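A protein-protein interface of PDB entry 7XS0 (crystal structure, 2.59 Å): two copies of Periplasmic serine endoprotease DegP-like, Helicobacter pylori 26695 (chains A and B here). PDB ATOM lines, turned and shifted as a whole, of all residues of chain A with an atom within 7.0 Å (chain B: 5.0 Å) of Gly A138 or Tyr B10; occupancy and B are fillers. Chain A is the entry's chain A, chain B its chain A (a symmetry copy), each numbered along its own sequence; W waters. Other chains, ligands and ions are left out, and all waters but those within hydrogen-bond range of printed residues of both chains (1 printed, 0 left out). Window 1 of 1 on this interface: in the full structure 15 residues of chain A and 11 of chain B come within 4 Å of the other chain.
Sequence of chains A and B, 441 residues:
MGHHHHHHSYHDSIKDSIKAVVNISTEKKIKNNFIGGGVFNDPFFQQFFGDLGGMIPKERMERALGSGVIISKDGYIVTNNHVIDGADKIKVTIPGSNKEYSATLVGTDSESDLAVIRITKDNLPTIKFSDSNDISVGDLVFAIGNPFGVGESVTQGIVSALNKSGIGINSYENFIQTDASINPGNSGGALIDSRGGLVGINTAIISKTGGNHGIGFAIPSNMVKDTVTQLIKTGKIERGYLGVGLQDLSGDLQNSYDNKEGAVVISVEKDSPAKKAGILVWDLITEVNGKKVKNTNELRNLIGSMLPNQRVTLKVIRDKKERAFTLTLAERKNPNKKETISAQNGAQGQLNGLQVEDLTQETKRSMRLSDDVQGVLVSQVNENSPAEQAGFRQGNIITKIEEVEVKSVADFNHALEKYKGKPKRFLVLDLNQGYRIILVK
O of Gly A138 is in hydrogen-bond range of N of Tyr B10, 2.8 Å away.
OD1 of Asp A139 is in hydrogen-bond range of OG of Ser B9, at 2.5 Å.
N of Leu A140 is in hydrogen-bond range of O of His B8, 2.9 Å away.
OE1 of Gln B156 is in hydrogen-bond range of NE2 of Gln A156 (3.4 Å).
The backbone NH of Ser A136 sits at hydrogen-bond distance from the side-chain carboxylate of Asp A139, at 2.4 Å.
O of Val A159 lies within hydrogen-bond range of N of Gly A138.
The backbone carbonyl oxygen of Ser B9 sits close to a ring nitrogen (NE2) of His B5 (3.3 Å).
A ring nitrogen (NE2) of His B5 is in hydrogen-bond range of the backbone NH of His B11 (3.4 Å).
NE2 of His B6 lies within hydrogen-bond range of OG of Ser B13 (2.6 Å).
The side-chain hydroxyl (OG) of Ser B9 lies within hydrogen-bond range of the backbone NH (N) of His B11, at 3.0 Å.
CD2 of His B11 touches CB of Ser A136, 3.4 Å away.
His B11 touches Val A137 (CD2 to O, 3.0 Å).
Ser B9 touches Gly A138.
Asp A139 touches His B8 (CA to O, 3.8 Å).
Leu A140 touches His B6.
Leu A140 touches Tyr B10 (CD2 to CE2, 3.9 Å).
Gln B156 touches Ile A158.
Of chain B, only Ser B9 (3.5 Å) and Tyr B10 (2.8 Å) come within 4 Å of Gly A138.
Of the printed residues of chain A, His B11 touches Ser A136 and Val A137.
Printed residues of chain B within 4 Å of Val A137: His B11 (3.0 Å).
The nearest printed residue of chain A that does not touch His B11 is Gly A138 (4.1 Å).
Hydrophobic or aromatic side chains of chain A within 4 Å of the printed part of chain B: Leu A140 and Ile A158.
Of the 12 printed residues of chain B, 6 touch a printed residue of chain A.
Among the printed residues, no Asp or Glu carboxylate lies within 4 Å of a Lys or Arg side-chain nitrogen of the other chain.
Leu A140 touches Tyr B10, but with the chains exchanged Tyr A10 does not touch Leu B140 (7.5 Å).
Gln B156 touches its own counterpart, Gln A156.
Positions printed for both chains: 10, 140 and 156.
Of the 11 pairs that touch across the chains among the printed residues, 1 has its exchanged pair printed and touching as well.
Water W1 lies within hydrogen-bond range of the backbone carbonyl oxygen (O) of Leu A140 (2.5 Å) and the backbone carbonyl oxygen (O) of His B8 (3.1 Å).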
ATOM      1  N   TYR A  10       3.745  26.249 -28.095  1.00  0.00           N
ATOM      2  CA  TYR A  10       3.058  26.203 -29.377  1.00  0.00           C
ATOM      3  C   TYR A  10       3.107  27.545 -30.095  1.00  0.00           C
ATOM      4  O   TYR A  10       2.408  27.727 -31.099  1.00  0.00           O
ATOM      5  CB  TYR A  10       1.604  25.771 -29.183  1.00  0.00           C
ATOM      6  CG  TYR A  10       1.450  24.396 -28.582  1.00  0.00           C
ATOM      7  CD1 TYR A  10       1.579  23.254 -29.362  1.00  0.00           C
ATOM      8  CD2 TYR A  10       1.162  24.239 -27.231  1.00  0.00           C
ATOM      9  CE1 TYR A  10       1.433  21.993 -28.812  1.00  0.00           C
ATOM     10  CE2 TYR A  10       1.013  22.985 -26.673  1.00  0.00           C
ATOM     11  CZ  TYR A  10       1.150  21.865 -27.466  1.00  0.00           C
ATOM     12  OH  TYR A  10       1.003  20.615 -26.914  1.00  0.00           O
ATOM     13  N   SER A 136      -9.752  14.844 -35.937  1.00  0.00           N
ATOM     14  CA  SER A 136     -10.100  13.711 -35.096  1.00  0.00           C
ATOM     15  C   SER A 136     -10.218  14.159 -33.650  1.00  0.00           C
ATOM     16  O   SER A 136      -9.601  15.144 -33.238  1.00  0.00           O
ATOM     17  CB  SER A 136      -9.053  12.592 -35.202  1.00  0.00           C
ATOM     18  OG  SER A 136      -9.008  12.054 -36.509  1.00  0.00           O
ATOM     19  N   VAL A 137     -11.027  13.426 -32.884  1.00  0.00           N
ATOM     20  CA  VAL A 137     -11.084  13.647 -31.446  1.00  0.00           C
ATOM     21  C   VAL A 137      -9.714  13.369 -30.848  1.00  0.00           C
ATOM     22  O   VAL A 137      -9.120  12.312 -31.084  1.00  0.00           O
ATOM     23  CB  VAL A 137     -12.168  12.763 -30.813  1.00  0.00           C
ATOM     24  CG1 VAL A 137     -12.108  12.859 -29.306  1.00  0.00           C
ATOM     25  CG2 VAL A 137     -13.543  13.173 -31.320  1.00  0.00           C
ATOM     26  N   GLY A 138      -9.203  14.316 -30.070  1.00  0.00           N
ATOM     27  CA  GLY A 138      -7.869  14.224 -29.525  1.00  0.00           C
ATOM     28  C   GLY A 138      -6.836  15.076 -30.233  1.00  0.00           C
ATOM     29  O   GLY A 138      -5.713  15.201 -29.726  1.00  0.00           O
ATOM     30  N   ASP A 139      -7.173  15.651 -31.388  1.00  0.00           N
ATOM     31  CA  ASP A 139      -6.281  16.604 -32.038  1.00  0.00           C
ATOM     32  C   ASP A 139      -6.127  17.845 -31.171  1.00  0.00           C
ATOM     33  O   ASP A 139      -7.098  18.342 -30.596  1.00  0.00           O
ATOM     34  CB  ASP A 139      -6.826  17.019 -33.407  1.00  0.00           C
ATOM     35  CG  ASP A 139      -6.876  15.876 -34.399  1.00  0.00           C
ATOM     36  OD1 ASP A 139      -6.108  14.908 -34.251  1.00  0.00           O
ATOM     37  OD2 ASP A 139      -7.679  15.964 -35.350  1.00  0.00           O
ATOM     38  N   LEU A 140      -4.903  18.356 -31.085  1.00  0.00           N
ATOM     39  CA  LEU A 140      -4.679  19.626 -30.404  1.00  0.00           C
ATOM     40  C   LEU A 140      -5.295  20.773 -31.198  1.00  0.00           C
ATOM     41  O   LEU A 140      -5.167  20.839 -32.423  1.00  0.00           O
ATOM     42  CB  LEU A 140      -3.182  19.871 -30.209  1.00  0.00           C
ATOM     43  CG  LEU A 140      -2.453  19.018 -29.170  1.00  0.00           C
ATOM     44  CD1 LEU A 140      -0.946  19.184 -29.311  1.00  0.00           C
ATOM     45  CD2 LEU A 140      -2.899  19.438 -27.779  1.00  0.00           C
ATOM     46  N   VAL A 141      -5.987  21.670 -30.492  1.00  0.00           N
ATOM     47  CA  VAL A 141      -6.592  22.850 -31.097  1.00  0.00           C
ATOM     48  C   VAL A 141      -6.387  24.040 -30.174  1.00  0.00           C
ATOM     49  O   VAL A 141      -6.202  23.900 -28.960  1.00  0.00           O
ATOM     50  CB  VAL A 141      -8.101  22.674 -31.383  1.00  0.00           C
ATOM     51  CG1 VAL A 141      -8.336  21.625 -32.465  1.00  0.00           C
ATOM     52  CG2 VAL A 141      -8.830  22.313 -30.106  1.00  0.00           C
ATOM     53  N   GLN A 156      -6.010  26.691 -25.086  1.00  0.00           N
ATOM     54  CA  GLN A 156      -5.522  25.421 -25.605  1.00  0.00           C
ATOM     55  C   GLN A 156      -6.443  24.283 -25.185  1.00  0.00           C
ATOM     56  O   GLN A 156      -6.943  24.261 -24.057  1.00  0.00           O
ATOM     57  CB  GLN A 156      -4.093  25.156 -25.112  1.00  0.00           C
ATOM     58  CG  GLN A 156      -3.488  23.838 -25.567  1.00  0.00           C
ATOM     59  CD  GLN A 156      -3.765  22.717 -24.583  1.00  0.00           C
ATOM     60  OE1 GLN A 156      -3.843  22.945 -23.374  1.00  0.00           O
ATOM     61  NE2 GLN A 156      -3.942  21.505 -25.094  1.00  0.00           N
ATOM     62  N   GLY A 157      -6.663  23.338 -26.094  1.00  0.00           N
ATOM     63  CA  GLY A 157      -7.395  22.134 -25.761  1.00  0.00           C
ATOM     64  C   GLY A 157      -7.289  21.084 -26.848  1.00  0.00           C
ATOM     65  O   GLY A 157      -6.351  21.101 -27.646  1.00  0.00           O
ATOM     66  N   ILE A 158      -8.255  20.170 -26.901  1.00  0.00           N
ATOM     67  CA  ILE A 158      -8.330  19.160 -27.948  1.00  0.00           C
ATOM     68  C   ILE A 158      -9.705  19.219 -28.600  1.00  0.00           C
ATOM     69  O   ILE A 158     -10.629  19.864 -28.103  1.00  0.00           O
ATOM     70  CB  ILE A 158      -8.066  17.734 -27.419  1.00  0.00           C
ATOM     71  CG1 ILE A 158      -9.131  17.345 -26.386  1.00  0.00           C
ATOM     72  CG2 ILE A 158      -6.653  17.608 -26.875  1.00  0.00           C
ATOM     73  CD1 ILE A 158      -9.082  15.891 -25.990  1.00  0.00           C
ATOM     74  N   VAL A 159      -9.827  18.532 -29.735  1.00  0.00           N
ATOM     75  CA  VAL A 159     -11.149  18.213 -30.262  1.00  0.00           C
ATOM     76  C   VAL A 159     -11.797  17.203 -29.324  1.00  0.00           C
ATOM     77  O   VAL A 159     -11.317  16.075 -29.182  1.00  0.00           O
ATOM     78  CB  VAL A 159     -11.060  17.677 -31.697  1.00  0.00           C
ATOM     79  CG1 VAL A 159     -12.435  17.263 -32.193  1.00  0.00           C
ATOM     80  CG2 VAL A 159     -10.454  18.719 -32.620  1.00  0.00           C
ATOM     81  N   SER A 160     -12.867  17.621 -28.649  1.00  0.00           N
ATOM     82  CA  SER A 160     -13.546  16.789 -27.667  1.00  0.00           C
ATOM     83  C   SER A 160     -14.601  15.894 -28.297  1.00  0.00           C
ATOM     84  O   SER A 160     -14.764  14.745 -27.876  1.00  0.00           O
ATOM     85  CB  SER A 160     -14.193  17.668 -26.590  1.00  0.00           C
ATOM     86  OG  SER A 160     -13.210  18.332 -25.818  1.00  0.00           O
ATOM     87  N   ALA A 161     -15.325  16.402 -29.291  1.00  0.00           N
ATOM     88  CA  ALA A 161     -16.362  15.625 -29.948  1.00  0.00           C
ATOM     89  C   ALA A 161     -16.598  16.200 -31.332  1.00  0.00           C
ATOM     90  O   ALA A 161     -16.385  17.391 -31.570  1.00  0.00           O
ATOM     91  CB  ALA A 161     -17.664  15.613 -29.139  1.00  0.00           C
ATOM     92  N   HIS B   5       3.667  11.458 -32.607  1.00  0.00           N
ATOM     93  CA  HIS B   5       2.248  11.708 -32.834  1.00  0.00           C
ATOM     94  C   HIS B   5       1.711  12.810 -31.929  1.00  0.00           C
ATOM     95  O   HIS B   5       0.846  13.588 -32.349  1.00  0.00           O
ATOM     96  CB  HIS B   5       1.457  10.410 -32.637  1.00  0.00           C
ATOM     97  CG  HIS B   5      -0.023  10.565 -32.810  1.00  0.00           C
ATOM     98  ND1 HIS B   5      -0.614  10.770 -34.038  1.00  0.00           N
ATOM     99  CD2 HIS B   5      -1.034  10.525 -31.910  1.00  0.00           C
ATOM    100  CE1 HIS B   5      -1.924  10.861 -33.887  1.00  0.00           C
ATOM    101  NE2 HIS B   5      -2.205  10.717 -32.603  1.00  0.00           N
ATOM    102  N   HIS B   6       2.220  12.915 -30.701  1.00  0.00           N
ATOM    103  CA  HIS B   6       1.629  13.797 -29.700  1.00  0.00           C
ATOM    104  C   HIS B   6       2.005  15.264 -29.869  1.00  0.00           C
ATOM    105  O   HIS B   6       1.535  16.094 -29.083  1.00  0.00           O
ATOM    106  CB  HIS B   6       2.008  13.329 -28.293  1.00  0.00           C
ATOM    107  CG  HIS B   6       1.347  12.049 -27.889  1.00  0.00           C
ATOM    108  ND1 HIS B   6       1.652  11.388 -26.720  1.00  0.00           N
ATOM    109  CD2 HIS B   6       0.401  11.304 -28.507  1.00  0.00           C
ATOM    110  CE1 HIS B   6       0.918  10.294 -26.630  1.00  0.00           C
ATOM    111  NE2 HIS B   6       0.151  10.219 -27.703  1.00  0.00           N
ATOM    112  N   HIS B   8       0.887  16.900 -32.268  1.00  0.00           N
ATOM    113  CA  HIS B   8      -0.252  17.448 -32.989  1.00  0.00           C
ATOM    114  C   HIS B   8      -1.563  16.813 -32.546  1.00  0.00           C
ATOM    115  O   HIS B   8      -2.625  17.433 -32.661  1.00  0.00           O
ATOM    116  CB  HIS B   8      -0.057  17.250 -34.493  1.00  0.00           C
ATOM    117  CG  HIS B   8       1.178  17.904 -35.030  1.00  0.00           C
ATOM    118  ND1 HIS B   8       1.293  19.269 -35.181  1.00  0.00           N
ATOM    119  CD2 HIS B   8       2.352  17.378 -35.454  1.00  0.00           C
ATOM    120  CE1 HIS B   8       2.486  19.556 -35.673  1.00  0.00           C
ATOM    121  NE2 HIS B   8       3.147  18.427 -35.849  1.00  0.00           N
ATOM    122  N   SER B   9      -1.509  15.584 -32.041  1.00  0.00           N
ATOM    123  CA  SER B   9      -2.743  14.882 -31.727  1.00  0.00           C
ATOM    124  C   SER B   9      -2.478  13.754 -30.742  1.00  0.00           C
ATOM    125  O   SER B   9      -1.375  13.209 -30.678  1.00  0.00           O
ATOM    126  CB  SER B   9      -3.394  14.317 -32.993  1.00  0.00           C
ATOM    127  OG  SER B   9      -4.586  13.621 -32.672  1.00  0.00           O
ATOM    128  N   TYR B  10      -3.518  13.412 -29.981  1.00  0.00           N
ATOM    129  CA  TYR B  10      -3.520  12.242 -29.115  1.00  0.00           C
ATOM    130  C   TYR B  10      -4.497  11.179 -29.600  1.00  0.00           C
ATOM    131  O   TYR B  10      -4.761  10.215 -28.873  1.00  0.00           O
ATOM    132  CB  TYR B  10      -3.863  12.647 -27.681  1.00  0.00           C
ATOM    133  CG  TYR B  10      -2.882  13.613 -27.066  1.00  0.00           C
ATOM    134  CD1 TYR B  10      -1.672  13.172 -26.545  1.00  0.00           C
ATOM    135  CD2 TYR B  10      -3.171  14.971 -26.996  1.00  0.00           C
ATOM    136  CE1 TYR B  10      -0.773  14.058 -25.978  1.00  0.00           C
ATOM    137  CE2 TYR B  10      -2.281  15.863 -26.432  1.00  0.00           C
ATOM    138  CZ  TYR B  10      -1.084  15.402 -25.924  1.00  0.00           C
ATOM    139  OH  TYR B  10      -0.195  16.288 -25.359  1.00  0.00           O
ATOM    140  N   HIS B  11      -5.036  11.335 -30.812  1.00  0.00           N
ATOM    141  CA  HIS B  11      -6.131  10.483 -31.264  1.00  0.00           C
ATOM    142  C   HIS B  11      -5.723   9.017 -31.351  1.00  0.00           C
ATOM    143  O   HIS B  11      -6.471   8.131 -30.923  1.00  0.00           O
ATOM    144  CB  HIS B  11      -6.654  10.971 -32.613  1.00  0.00           C
ATOM    145  CG  HIS B  11      -7.717  10.094 -33.191  1.00  0.00           C
ATOM    146  ND1 HIS B  11      -7.439   9.095 -34.100  1.00  0.00           N
ATOM    147  CD2 HIS B  11      -9.049  10.024 -32.952  1.00  0.00           C
ATOM    148  CE1 HIS B  11      -8.559   8.474 -34.424  1.00  0.00           C
ATOM    149  NE2 HIS B  11      -9.550   9.017 -33.741  1.00  0.00           N
ATOM    150  N   ASP B  12      -4.548   8.737 -31.923  1.00  0.00           N
ATOM    151  CA  ASP B  12      -4.142   7.344 -32.085  1.00  0.00           C
ATOM    152  C   ASP B  12      -3.908   6.671 -30.741  1.00  0.00           C
ATOM    153  O   ASP B  12      -4.074   5.454 -30.621  1.00  0.00           O
ATOM    154  CB  ASP B  12      -2.888   7.249 -32.955  1.00  0.00           C
ATOM    155  CG  ASP B  12      -3.158   7.587 -34.409  1.00  0.00           C
ATOM    156  OD1 ASP B  12      -4.304   7.384 -34.863  1.00  0.00           O
ATOM    157  OD2 ASP B  12      -2.225   8.043 -35.104  1.00  0.00           O
ATOM    158  N   SER B  13      -3.528   7.444 -29.725  1.00  0.00           N
ATOM    159  CA  SER B  13      -3.278   6.892 -28.400  1.00  0.00           C
ATOM    160  C   SER B  13      -4.555   6.596 -27.624  1.00  0.00           C
ATOM    161  O   SER B  13      -4.518   5.788 -26.690  1.00  0.00           O
ATOM    162  CB  SER B  13      -2.402   7.852 -27.595  1.00  0.00           C
ATOM    163  OG  SER B  13      -1.134   8.015 -28.204  1.00  0.00           O
ATOM    164  N   ILE B  14      -5.676   7.220 -27.977  1.00  0.00           N
ATOM    165  CA  ILE B  14      -6.902   7.110 -27.195  1.00  0.00           C
ATOM    166  C   ILE B  14      -8.046   6.469 -27.967  1.00  0.00           C
ATOM    167  O   ILE B  14      -9.111   6.220 -27.375  1.00  0.00           O
ATOM    168  CB  ILE B  14      -7.344   8.487 -26.658  1.00  0.00           C
ATOM    169  CG1 ILE B  14      -7.748   9.397 -27.816  1.00  0.00           C
ATOM    170  CG2 ILE B  14      -6.214   9.131 -25.877  1.00  0.00           C
ATOM    171  CD1 ILE B  14      -8.405  10.682 -27.376  1.00  0.00           C
ATOM    172  N   LEU B 140      -0.089  13.315 -18.394  1.00  0.00           N
ATOM    173  CA  LEU B 140      -1.224  13.601 -19.263  1.00  0.00           C
ATOM    174  C   LEU B 140      -2.323  12.565 -19.063  1.00  0.00           C
ATOM    175  O   LEU B 140      -2.058  11.363 -18.976  1.00  0.00           O
ATOM    176  CB  LEU B 140      -0.783  13.618 -20.729  1.00  0.00           C
ATOM    177  CG  LEU B 140       0.064  14.801 -21.201  1.00  0.00           C
ATOM    178  CD1 LEU B 140       0.649  14.518 -22.577  1.00  0.00           C
ATOM    179  CD2 LEU B 140      -0.803  16.049 -21.245  1.00  0.00           C
ATOM    180  N   PHE B 142      -6.759  11.819 -20.084  1.00  0.00           N
ATOM    181  CA  PHE B 142      -7.930  12.230 -20.845  1.00  0.00           C
ATOM    182  C   PHE B 142      -9.155  11.565 -20.236  1.00  0.00           C
ATOM    183  O   PHE B 142      -9.124  10.372 -19.915  1.00  0.00           O
ATOM    184  CB  PHE B 142      -7.869  11.904 -22.361  1.00  0.00           C
ATOM    185  CG  PHE B 142      -6.550  12.240 -23.039  1.00  0.00           C
ATOM    186  CD1 PHE B 142      -5.327  11.892 -22.484  1.00  0.00           C
ATOM    187  CD2 PHE B 142      -6.541  13.094 -24.124  1.00  0.00           C
ATOM    188  CE1 PHE B 142      -4.141  12.238 -23.075  1.00  0.00           C
ATOM    189  CE2 PHE B 142      -5.349  13.474 -24.708  1.00  0.00           C
ATOM    190  CZ  PHE B 142      -4.147  13.041 -24.175  1.00  0.00           C
ATOM    191  N   GLN B 156      -9.059  16.837 -22.108  1.00  0.00           N
ATOM    192  CA  GLN B 156      -7.630  16.657 -21.898  1.00  0.00           C
ATOM    193  C   GLN B 156      -7.168  17.437 -20.675  1.00  0.00           C
ATOM    194  O   GLN B 156      -7.623  18.558 -20.432  1.00  0.00           O
ATOM    195  CB  GLN B 156      -6.846  17.106 -23.139  1.00  0.00           C
ATOM    196  CG  GLN B 156      -5.335  16.993 -23.023  1.00  0.00           C
ATOM    197  CD  GLN B 156      -4.711  18.265 -22.481  1.00  0.00           C
ATOM    198  OE1 GLN B 156      -5.204  19.366 -22.735  1.00  0.00           O
ATOM    199  NE2 GLN B 156      -3.640  18.122 -21.710  1.00  0.00           N
HETATM  200  O   HOH W   1      -4.370  19.393 -34.366  1.00  0.00           O
